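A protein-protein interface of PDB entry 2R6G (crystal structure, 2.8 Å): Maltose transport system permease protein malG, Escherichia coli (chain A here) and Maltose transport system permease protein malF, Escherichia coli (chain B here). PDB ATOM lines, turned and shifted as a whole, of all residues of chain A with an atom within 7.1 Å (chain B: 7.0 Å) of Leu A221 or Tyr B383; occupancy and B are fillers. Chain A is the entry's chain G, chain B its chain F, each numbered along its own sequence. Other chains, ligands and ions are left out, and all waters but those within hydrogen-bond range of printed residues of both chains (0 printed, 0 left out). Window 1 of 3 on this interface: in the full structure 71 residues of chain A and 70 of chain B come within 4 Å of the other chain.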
ATOM      1  N   ALA A  96     -26.043  27.268 -19.321  1.00  0.00           N
ATOM      2  CA  ALA A  96     -24.799  27.014 -18.600  1.00  0.00           C
ATOM      3  C   ALA A  96     -25.061  26.618 -17.149  1.00  0.00           C
ATOM      4  O   ALA A  96     -24.525  25.614 -16.681  1.00  0.00           O
ATOM      5  CB  ALA A  96     -23.875  28.222 -18.677  1.00  0.00           C
ATOM      6  N   LEU A 172     -18.329  15.415 -20.896  1.00  0.00           N
ATOM      7  CA  LEU A 172     -17.041  16.106 -20.891  1.00  0.00           C
ATOM      8  C   LEU A 172     -16.776  16.779 -19.541  1.00  0.00           C
ATOM      9  O   LEU A 172     -15.709  16.598 -18.953  1.00  0.00           O
ATOM     10  CB  LEU A 172     -16.957  17.130 -22.044  1.00  0.00           C
ATOM     11  CG  LEU A 172     -17.881  18.371 -22.105  1.00  0.00           C
ATOM     12  CD1 LEU A 172     -17.236  19.533 -22.876  1.00  0.00           C
ATOM     13  CD2 LEU A 172     -19.267  18.053 -22.676  1.00  0.00           C
ATOM     14  N   HIS A 173     -17.768  17.521 -19.049  1.00  0.00           N
ATOM     15  CA  HIS A 173     -17.626  18.326 -17.839  1.00  0.00           C
ATOM     16  C   HIS A 173     -17.615  17.495 -16.560  1.00  0.00           C
ATOM     17  O   HIS A 173     -16.840  17.783 -15.651  1.00  0.00           O
ATOM     18  CB  HIS A 173     -18.708  19.406 -17.772  1.00  0.00           C
ATOM     19  CG  HIS A 173     -18.665  20.370 -18.916  1.00  0.00           C
ATOM     20  ND1 HIS A 173     -19.708  20.520 -19.804  1.00  0.00           N
ATOM     21  CD2 HIS A 173     -17.697  21.225 -19.326  1.00  0.00           C
ATOM     22  CE1 HIS A 173     -19.390  21.432 -20.706  1.00  0.00           C
ATOM     23  NE2 HIS A 173     -18.174  21.875 -20.439  1.00  0.00           N
ATOM     24  N   THR A 176     -14.305  16.330 -15.910  1.00  0.00           N
ATOM     25  CA  THR A 176     -13.468  17.467 -15.537  1.00  0.00           C
ATOM     26  C   THR A 176     -13.627  17.820 -14.065  1.00  0.00           C
ATOM     27  O   THR A 176     -12.654  17.779 -13.309  1.00  0.00           O
ATOM     28  CB  THR A 176     -13.769  18.709 -16.407  1.00  0.00           C
ATOM     29  OG1 THR A 176     -13.756  18.344 -17.792  1.00  0.00           O
ATOM     30  CG2 THR A 176     -12.735  19.805 -16.166  1.00  0.00           C
ATOM     31  N   LEU A 215     -15.733  25.345 -11.471  1.00  0.00           N
ATOM     32  CA  LEU A 215     -17.143  25.606 -11.733  1.00  0.00           C
ATOM     33  C   LEU A 215     -17.279  26.777 -12.703  1.00  0.00           C
ATOM     34  O   LEU A 215     -18.153  26.777 -13.569  1.00  0.00           O
ATOM     35  CB  LEU A 215     -17.901  25.903 -10.435  1.00  0.00           C
ATOM     36  CG  LEU A 215     -18.014  24.854  -9.320  1.00  0.00           C
ATOM     37  CD1 LEU A 215     -18.878  25.394  -8.185  1.00  0.00           C
ATOM     38  CD2 LEU A 215     -18.582  23.537  -9.823  1.00  0.00           C
ATOM     39  N   ALA A 216     -16.404  27.770 -12.551  1.00  0.00           N
ATOM     40  CA  ALA A 216     -16.376  28.920 -13.452  1.00  0.00           C
ATOM     41  C   ALA A 216     -15.881  28.520 -14.840  1.00  0.00           C
ATOM     42  O   ALA A 216     -16.375  29.032 -15.843  1.00  0.00           O
ATOM     43  CB  ALA A 216     -15.523  30.041 -12.872  1.00  0.00           C
ATOM     44  N   VAL A 217     -14.913  27.603 -14.888  1.00  0.00           N
ATOM     45  CA  VAL A 217     -14.423  27.029 -16.147  1.00  0.00           C
ATOM     46  C   VAL A 217     -15.577  26.389 -16.927  1.00  0.00           C
ATOM     47  O   VAL A 217     -15.841  26.752 -18.076  1.00  0.00           O
ATOM     48  CB  VAL A 217     -13.296  25.981 -15.908  1.00  0.00           C
ATOM     49  CG1 VAL A 217     -12.915  25.274 -17.201  1.00  0.00           C
ATOM     50  CG2 VAL A 217     -12.075  26.642 -15.300  1.00  0.00           C
ATOM     51  N   VAL A 218     -16.264  25.452 -16.279  1.00  0.00           N
ATOM     52  CA  VAL A 218     -17.419  24.780 -16.863  1.00  0.00           C
ATOM     53  C   VAL A 218     -18.487  25.788 -17.307  1.00  0.00           C
ATOM     54  O   VAL A 218     -19.003  25.695 -18.425  1.00  0.00           O
ATOM     55  CB  VAL A 218     -18.005  23.712 -15.895  1.00  0.00           C
ATOM     56  CG1 VAL A 218     -19.361  23.202 -16.377  1.00  0.00           C
ATOM     57  CG2 VAL A 218     -17.034  22.552 -15.736  1.00  0.00           C
ATOM     58  N   PHE A 219     -18.795  26.762 -16.452  1.00  0.00           N
ATOM     59  CA  PHE A 219     -19.797  27.771 -16.793  1.00  0.00           C
ATOM     60  C   PHE A 219     -19.435  28.528 -18.062  1.00  0.00           C
ATOM     61  O   PHE A 219     -20.247  28.608 -18.985  1.00  0.00           O
ATOM     62  CB  PHE A 219     -20.043  28.757 -15.648  1.00  0.00           C
ATOM     63  CG  PHE A 219     -21.129  29.760 -15.941  1.00  0.00           C
ATOM     64  CD1 PHE A 219     -22.437  29.522 -15.542  1.00  0.00           C
ATOM     65  CD2 PHE A 219     -20.847  30.934 -16.632  1.00  0.00           C
ATOM     66  CE1 PHE A 219     -23.452  30.445 -15.814  1.00  0.00           C
ATOM     67  CE2 PHE A 219     -21.855  31.861 -16.915  1.00  0.00           C
ATOM     68  CZ  PHE A 219     -23.158  31.613 -16.504  1.00  0.00           C
ATOM     69  N   ILE A 220     -18.226  29.083 -18.109  1.00  0.00           N
ATOM     70  CA  ILE A 220     -17.819  29.888 -19.263  1.00  0.00           C
ATOM     71  C   ILE A 220     -17.700  29.061 -20.543  1.00  0.00           C
ATOM     72  O   ILE A 220     -18.159  29.496 -21.594  1.00  0.00           O
ATOM     73  CB  ILE A 220     -16.564  30.782 -18.997  1.00  0.00           C
ATOM     74  CG1 ILE A 220     -15.309  29.952 -18.711  1.00  0.00           C
ATOM     75  CG2 ILE A 220     -16.844  31.763 -17.856  1.00  0.00           C
ATOM     76  CD1 ILE A 220     -14.081  30.789 -18.358  1.00  0.00           C
ATOM     77  N   LEU A 221     -17.129  27.860 -20.443  1.00  0.00           N
ATOM     78  CA  LEU A 221     -17.043  26.945 -21.589  1.00  0.00           C
ATOM     79  C   LEU A 221     -18.413  26.615 -22.181  1.00  0.00           C
ATOM     80  O   LEU A 221     -18.578  26.598 -23.403  1.00  0.00           O
ATOM     81  CB  LEU A 221     -16.309  25.655 -21.215  1.00  0.00           C
ATOM     82  CG  LEU A 221     -14.779  25.705 -21.171  1.00  0.00           C
ATOM     83  CD1 LEU A 221     -14.219  24.420 -20.587  1.00  0.00           C
ATOM     84  CD2 LEU A 221     -14.183  25.968 -22.549  1.00  0.00           C
ATOM     85  N   SER A 222     -19.383  26.358 -21.306  1.00  0.00           N
ATOM     86  CA  SER A 222     -20.756  26.082 -21.719  1.00  0.00           C
ATOM     87  C   SER A 222     -21.459  27.334 -22.229  1.00  0.00           C
ATOM     88  O   SER A 222     -22.224  27.271 -23.196  1.00  0.00           O
ATOM     89  CB  SER A 222     -21.550  25.472 -20.565  1.00  0.00           C
ATOM     90  OG  SER A 222     -20.951  24.264 -20.133  1.00  0.00           O
ATOM     91  N   PHE A 223     -21.198  28.466 -21.579  1.00  0.00           N
ATOM     92  CA  PHE A 223     -21.791  29.732 -21.991  1.00  0.00           C
ATOM     93  C   PHE A 223     -21.373  30.081 -23.412  1.00  0.00           C
ATOM     94  O   PHE A 223     -22.207  30.493 -24.212  1.00  0.00           O
ATOM     95  CB  PHE A 223     -21.426  30.864 -21.028  1.00  0.00           C
ATOM     96  CG  PHE A 223     -22.109  32.166 -21.340  1.00  0.00           C
ATOM     97  CD1 PHE A 223     -23.388  32.427 -20.861  1.00  0.00           C
ATOM     98  CD2 PHE A 223     -21.476  33.131 -22.116  1.00  0.00           C
ATOM     99  CE1 PHE A 223     -24.026  33.630 -21.147  1.00  0.00           C
ATOM    100  CE2 PHE A 223     -22.108  34.339 -22.411  1.00  0.00           C
ATOM    101  CZ  PHE A 223     -23.386  34.587 -21.924  1.00  0.00           C
ATOM    102  N   ILE A 224     -20.088  29.906 -23.725  1.00  0.00           N
ATOM    103  CA  ILE A 224     -19.602  30.186 -25.078  1.00  0.00           C
ATOM    104  C   ILE A 224     -20.127  29.157 -26.078  1.00  0.00           C
ATOM    105  O   ILE A 224     -20.500  29.517 -27.190  1.00  0.00           O
ATOM    106  CB  ILE A 224     -18.033  30.369 -25.187  1.00  0.00           C
ATOM    107  CG1 ILE A 224     -17.300  29.048 -25.432  1.00  0.00           C
ATOM    108  CG2 ILE A 224     -17.452  31.145 -24.001  1.00  0.00           C
ATOM    109  CD1 ILE A 224     -17.141  28.717 -26.909  1.00  0.00           C
ATOM    110  N   ALA A 225     -20.173  27.890 -25.668  1.00  0.00           N
ATOM    111  CA  ALA A 225     -20.629  26.807 -26.544  1.00  0.00           C
ATOM    112  C   ALA A 225     -22.041  27.071 -27.052  1.00  0.00           C
ATOM    113  O   ALA A 225     -22.348  26.813 -28.216  1.00  0.00           O
ATOM    114  CB  ALA A 225     -20.564  25.468 -25.826  1.00  0.00           C
ATOM    115  N   ALA A 226     -22.882  27.607 -26.171  1.00  0.00           N
ATOM    116  CA  ALA A 226     -24.272  27.897 -26.493  1.00  0.00           C
ATOM    117  C   ALA A 226     -24.440  29.200 -27.275  1.00  0.00           C
ATOM    118  O   ALA A 226     -25.318  29.299 -28.132  1.00  0.00           O
ATOM    119  CB  ALA A 226     -25.108  27.914 -25.227  1.00  0.00           C
ATOM    120  N   VAL A 277     -18.834  37.699 -19.411  1.00  0.00           N
ATOM    121  CA  VAL A 277     -18.940  36.472 -18.621  1.00  0.00           C
ATOM    122  C   VAL A 277     -17.558  35.947 -18.219  1.00  0.00           C
ATOM    123  O   VAL A 277     -17.382  35.441 -17.108  1.00  0.00           O
ATOM    124  CB  VAL A 277     -19.798  35.394 -19.349  1.00  0.00           C
ATOM    125  CG1 VAL A 277     -19.505  33.995 -18.840  1.00  0.00           C
ATOM    126  CG2 VAL A 277     -21.277  35.709 -19.189  1.00  0.00           C
ATOM    127  N   THR B 295      -2.222  22.637 -28.928  1.00  0.00           N
ATOM    128  CA  THR B 295      -3.352  23.262 -28.249  1.00  0.00           C
ATOM    129  C   THR B 295      -3.169  23.232 -26.728  1.00  0.00           C
ATOM    130  O   THR B 295      -3.368  24.245 -26.057  1.00  0.00           O
ATOM    131  CB  THR B 295      -4.681  22.591 -28.682  1.00  0.00           C
ATOM    132  OG1 THR B 295      -4.892  22.820 -30.080  1.00  0.00           O
ATOM    133  CG2 THR B 295      -5.863  23.144 -27.924  1.00  0.00           C
ATOM    134  N   GLY B 299      -1.815  26.347 -24.638  1.00  0.00           N
ATOM    135  CA  GLY B 299      -2.837  26.600 -23.629  1.00  0.00           C
ATOM    136  C   GLY B 299      -2.282  26.652 -22.220  1.00  0.00           C
ATOM    137  O   GLY B 299      -2.524  27.614 -21.489  1.00  0.00           O
ATOM    138  N   LEU B 321      -6.249  36.900 -25.016  1.00  0.00           N
ATOM    139  CA  LEU B 321      -5.850  35.571 -25.475  1.00  0.00           C
ATOM    140  C   LEU B 321      -7.066  34.667 -25.684  1.00  0.00           C
ATOM    141  O   LEU B 321      -6.968  33.604 -26.300  1.00  0.00           O
ATOM    142  CB  LEU B 321      -4.879  34.934 -24.477  1.00  0.00           C
ATOM    143  CG  LEU B 321      -3.490  35.565 -24.322  1.00  0.00           C
ATOM    144  CD1 LEU B 321      -2.913  35.263 -22.951  1.00  0.00           C
ATOM    145  CD2 LEU B 321      -2.543  35.099 -25.420  1.00  0.00           C
ATOM    146  N   ILE B 322      -8.210  35.111 -25.174  1.00  0.00           N
ATOM    147  CA  ILE B 322      -9.449  34.339 -25.206  1.00  0.00           C
ATOM    148  C   ILE B 322     -10.333  34.650 -26.415  1.00  0.00           C
ATOM    149  O   ILE B 322     -11.141  33.817 -26.832  1.00  0.00           O
ATOM    150  CB  ILE B 322     -10.217  34.500 -23.858  1.00  0.00           C
ATOM    151  CG1 ILE B 322     -10.144  33.201 -23.055  1.00  0.00           C
ATOM    152  CG2 ILE B 322     -11.680  34.924 -24.058  1.00  0.00           C
ATOM    153  CD1 ILE B 322      -8.767  32.864 -22.517  1.00  0.00           C
ATOM    154  N   TYR B 325     -11.758  32.642 -29.299  1.00  0.00           N
ATOM    155  CA  TYR B 325     -12.823  31.712 -28.922  1.00  0.00           C
ATOM    156  C   TYR B 325     -14.151  32.447 -28.717  1.00  0.00           C
ATOM    157  O   TYR B 325     -15.223  31.843 -28.799  1.00  0.00           O
ATOM    158  CB  TYR B 325     -12.422  30.961 -27.651  1.00  0.00           C
ATOM    159  CG  TYR B 325     -13.062  29.602 -27.450  1.00  0.00           C
ATOM    160  CD1 TYR B 325     -13.381  28.781 -28.534  1.00  0.00           C
ATOM    161  CD2 TYR B 325     -13.308  29.120 -26.164  1.00  0.00           C
ATOM    162  CE1 TYR B 325     -13.959  27.529 -28.340  1.00  0.00           C
ATOM    163  CE2 TYR B 325     -13.876  27.867 -25.960  1.00  0.00           C
ATOM    164  CZ  TYR B 325     -14.197  27.077 -27.053  1.00  0.00           C
ATOM    165  OH  TYR B 325     -14.766  25.843 -26.850  1.00  0.00           O
ATOM    166  N   LEU B 379      -7.436  28.446 -33.209  1.00  0.00           N
ATOM    167  CA  LEU B 379      -8.853  28.218 -32.985  1.00  0.00           C
ATOM    168  C   LEU B 379      -9.137  27.488 -31.671  1.00  0.00           C
ATOM    169  O   LEU B 379     -10.206  27.663 -31.076  1.00  0.00           O
ATOM    170  CB  LEU B 379      -9.420  27.422 -34.162  1.00  0.00           C
ATOM    171  CG  LEU B 379     -10.887  27.579 -34.563  1.00  0.00           C
ATOM    172  CD1 LEU B 379     -11.311  29.044 -34.683  1.00  0.00           C
ATOM    173  CD2 LEU B 379     -11.120  26.840 -35.872  1.00  0.00           C
ATOM    174  N   GLY B 380      -8.177  26.685 -31.218  1.00  0.00           N
ATOM    175  CA  GLY B 380      -8.406  25.775 -30.102  1.00  0.00           C
ATOM    176  C   GLY B 380      -7.613  25.998 -28.829  1.00  0.00           C
ATOM    177  O   GLY B 380      -7.949  25.419 -27.793  1.00  0.00           O
ATOM    178  N   TYR B 381      -6.568  26.823 -28.888  1.00  0.00           N
ATOM    179  CA  TYR B 381      -5.733  27.071 -27.706  1.00  0.00           C
ATOM    180  C   TYR B 381      -6.496  27.714 -26.530  1.00  0.00           C
ATOM    181  O   TYR B 381      -6.250  27.342 -25.379  1.00  0.00           O
ATOM    182  CB  TYR B 381      -4.437  27.843 -28.047  1.00  0.00           C
ATOM    183  CG  TYR B 381      -4.574  29.351 -28.078  1.00  0.00           C
ATOM    184  CD1 TYR B 381      -4.579  30.094 -26.895  1.00  0.00           C
ATOM    185  CD2 TYR B 381      -4.700  30.037 -29.284  1.00  0.00           C
ATOM    186  CE1 TYR B 381      -4.720  31.471 -26.910  1.00  0.00           C
ATOM    187  CE2 TYR B 381      -4.836  31.423 -29.311  1.00  0.00           C
ATOM    188  CZ  TYR B 381      -4.844  32.131 -28.118  1.00  0.00           C
ATOM    189  OH  TYR B 381      -4.980  33.497 -28.121  1.00  0.00           O
ATOM    190  N   PRO B 382      -7.418  28.672 -26.804  1.00  0.00           N
ATOM    191  CA  PRO B 382      -8.137  29.279 -25.678  1.00  0.00           C
ATOM    192  C   PRO B 382      -9.022  28.291 -24.918  1.00  0.00           C
ATOM    193  O   PRO B 382      -9.310  28.508 -23.741  1.00  0.00           O
ATOM    194  CB  PRO B 382      -8.984  30.370 -26.338  1.00  0.00           C
ATOM    195  CG  PRO B 382      -9.102  29.962 -27.749  1.00  0.00           C
ATOM    196  CD  PRO B 382      -7.842  29.258 -28.089  1.00  0.00           C
ATOM    197  N   TYR B 383      -9.439  27.218 -25.586  1.00  0.00           N
ATOM    198  CA  TYR B 383     -10.166  26.136 -24.928  1.00  0.00           C
ATOM    199  C   TYR B 383      -9.328  25.486 -23.826  1.00  0.00           C
ATOM    200  O   TYR B 383      -9.819  25.277 -22.717  1.00  0.00           O
ATOM    201  CB  TYR B 383     -10.618  25.083 -25.946  1.00  0.00           C
ATOM    202  CG  TYR B 383     -11.263  23.862 -25.328  1.00  0.00           C
ATOM    203  CD1 TYR B 383     -12.568  23.914 -24.841  1.00  0.00           C
ATOM    204  CD2 TYR B 383     -10.572  22.652 -25.236  1.00  0.00           C
ATOM    205  CE1 TYR B 383     -13.167  22.798 -24.268  1.00  0.00           C
ATOM    206  CE2 TYR B 383     -11.165  21.527 -24.666  1.00  0.00           C
ATOM    207  CZ  TYR B 383     -12.462  21.610 -24.185  1.00  0.00           C
ATOM    208  OH  TYR B 383     -13.058  20.508 -23.623  1.00  0.00           O
ATOM    209  N   MET B 384      -8.070  25.176 -24.134  1.00  0.00           N
ATOM    210  CA  MET B 384      -7.184  24.522 -23.173  1.00  0.00           C
ATOM    211  C   MET B 384      -6.721  25.460 -22.065  1.00  0.00           C
ATOM    212  O   MET B 384      -6.565  25.037 -20.921  1.00  0.00           O
ATOM    213  CB  MET B 384      -5.981  23.877 -23.865  1.00  0.00           C
ATOM    214  CG  MET B 384      -6.323  22.647 -24.698  1.00  0.00           C
ATOM    215  SD  MET B 384      -7.034  21.265 -23.775  1.00  0.00           S
ATOM    216  CE  MET B 384      -7.656  20.257 -25.118  1.00  0.00           C
ATOM    217  N   MET B 385      -6.504  26.729 -22.398  1.00  0.00           N
ATOM    218  CA  MET B 385      -6.030  27.674 -21.394  1.00  0.00           C
ATOM    219  C   MET B 385      -7.128  28.072 -20.405  1.00  0.00           C
ATOM    220  O   MET B 385      -6.844  28.280 -19.227  1.00  0.00           O
ATOM    221  CB  MET B 385      -5.320  28.888 -22.017  1.00  0.00           C
ATOM    222  CG  MET B 385      -6.204  29.998 -22.553  1.00  0.00           C
ATOM    223  SD  MET B 385      -5.321  31.573 -22.539  1.00  0.00           S
ATOM    224  CE  MET B 385      -5.447  32.032 -20.812  1.00  0.00           C
ATOM    225  N   ILE B 386      -8.370  28.162 -20.881  1.00  0.00           N
ATOM    226  CA  ILE B 386      -9.522  28.360 -19.998  1.00  0.00           C
ATOM    227  C   ILE B 386      -9.619  27.166 -19.049  1.00  0.00           C
ATOM    228  O   ILE B 386      -9.796  27.326 -17.835  1.00  0.00           O
ATOM    229  CB  ILE B 386     -10.845  28.532 -20.794  1.00  0.00           C
ATOM    230  CG1 ILE B 386     -10.964  29.963 -21.336  1.00  0.00           C
ATOM    231  CG2 ILE B 386     -12.059  28.195 -19.927  1.00  0.00           C
ATOM    232  CD1 ILE B 386     -12.028  30.147 -22.418  1.00  0.00           C
ATOM    233  N   LEU B 387      -9.481  25.977 -19.629  1.00  0.00           N
ATOM    234  CA  LEU B 387      -9.491  24.717 -18.902  1.00  0.00           C
ATOM    235  C   LEU B 387      -8.389  24.708 -17.844  1.00  0.00           C
ATOM    236  O   LEU B 387      -8.654  24.440 -16.672  1.00  0.00           O
ATOM    237  CB  LEU B 387      -9.283  23.572 -19.894  1.00  0.00           C
ATOM    238  CG  LEU B 387      -9.835  22.179 -19.624  1.00  0.00           C
ATOM    239  CD1 LEU B 387     -11.347  22.161 -19.743  1.00  0.00           C
ATOM    240  CD2 LEU B 387      -9.215  21.233 -20.630  1.00  0.00           C
ATOM    241  N   CYS B 388      -7.166  25.028 -18.265  1.00  0.00           N
ATOM    242  CA  CYS B 388      -6.012  25.061 -17.370  1.00  0.00           C
ATOM    243  C   CYS B 388      -6.069  26.178 -16.335  1.00  0.00           C
ATOM    244  O   CYS B 388      -5.568  26.012 -15.225  1.00  0.00           O
ATOM    245  CB  CYS B 388      -4.717  25.160 -18.165  1.00  0.00           C
ATOM    246  SG  CYS B 388      -4.203  23.600 -18.867  1.00  0.00           S
ATOM    247  N   LEU B 429      -9.580  15.029 -21.196  1.00  0.00           N
ATOM    248  CA  LEU B 429      -9.936  16.216 -21.964  1.00  0.00           C
ATOM    249  C   LEU B 429      -9.215  16.317 -23.303  1.00  0.00           C
ATOM    250  O   LEU B 429      -9.711  16.962 -24.228  1.00  0.00           O
ATOM    251  CB  LEU B 429      -9.698  17.473 -21.128  1.00  0.00           C
ATOM    252  CG  LEU B 429     -10.736  17.666 -20.023  1.00  0.00           C
ATOM    253  CD1 LEU B 429     -10.126  18.301 -18.788  1.00  0.00           C
ATOM    254  CD2 LEU B 429     -11.925  18.468 -20.533  1.00  0.00           C
ATOM    255  N   MET B 430      -8.053  15.678 -23.409  1.00  0.00           N
ATOM    256  CA  MET B 430      -7.280  15.714 -24.652  1.00  0.00           C
ATOM    257  C   MET B 430      -7.450  14.472 -25.536  1.00  0.00           C
ATOM    258  O   MET B 430      -7.165  14.522 -26.737  1.00  0.00           O
ATOM    259  CB  MET B 430      -5.804  16.039 -24.388  1.00  0.00           C
ATOM    260  CG  MET B 430      -5.102  15.157 -23.370  1.00  0.00           C
ATOM    261  SD  MET B 430      -3.650  15.983 -22.675  1.00  0.00           S
ATOM    262  CE  MET B 430      -2.516  15.953 -24.066  1.00  0.00           C
ATOM    263  N   ALA B 432     -10.519  13.266 -25.685  1.00  0.00           N
ATOM    264  CA  ALA B 432     -11.800  13.735 -26.207  1.00  0.00           C
ATOM    265  C   ALA B 432     -11.569  14.796 -27.272  1.00  0.00           C
ATOM    266  O   ALA B 432     -12.312  14.877 -28.251  1.00  0.00           O
ATOM    267  CB  ALA B 432     -12.666  14.283 -25.089  1.00  0.00           C
ATOM    268  N   SER B 433     -10.530  15.604 -27.076  1.00  0.00           N
ATOM    269  CA  SER B 433     -10.141  16.605 -28.059  1.00  0.00           C
ATOM    270  C   SER B 433      -9.543  15.948 -29.298  1.00  0.00           C
ATOM    271  O   SER B 433      -9.655  16.484 -30.402  1.00  0.00           O
ATOM    272  CB  SER B 433      -9.149  17.598 -27.462  1.00  0.00           C
ATOM    273  OG  SER B 433      -8.918  18.669 -28.360  1.00  0.00           O
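Of the printed residues of chain B, Thr A176 touches Leu B429 (3.3 Å).
Printed residues of chain B within 4 Å of Ile A220: Ile B386.
Of chain B, only Tyr B325, Tyr B383, Ile B386 and Leu B387 come within 4 Å of Leu A221.
Of the printed residues of chain B, Ile A224 touches Tyr B325.
Of the printed residues of chain A, Tyr B325 touches Leu A221 and Ile A224.
Of the 17 printed residues of chain A, 5 touch a printed residue of chain B.
Hydrophobic or aromatic side chains of chain A within 4 Å of the printed part of chain B: Val A217, Ile A220, Leu A221 and Ile A224.
Along chain A the printed residues that touch a printed residue of chain B span positions 176 to 224.
Hydrophobic or aromatic side chains of chain B that line the printed part of chain A: Tyr B325, Tyr B383, Ile B386, Leu B387 and Leu B429.
Along chain B the printed residues that touch a printed residue of chain A span positions 325 to 429.
Among the printed residues, no Asp or Glu carboxylate lies within 4 Å of a Lys or Arg side-chain nitrogen of the other chain.
OG1 of Thr A176 sits at hydrogen-bond distance from O of Leu A172 (2.9 Å).
Among the printed residues, merely in contact across the chains: Thr A176 with Leu B429 (3.3 Å), Val A217 with Ile B386 (3.5 Å), Val A217 with Leu B387 (3.9 Å), Ile A220 with Ile B386 (3.6 Å), Leu A221 with Tyr B325 (3.9 Å), Leu A221 with Tyr B383 (3.5 Å), Leu A221 with Ile B386 (3.9 Å), Leu A221 with Leu B387 (3.8 Å) and Ile A224 with Tyr B325 (3.4 Å).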
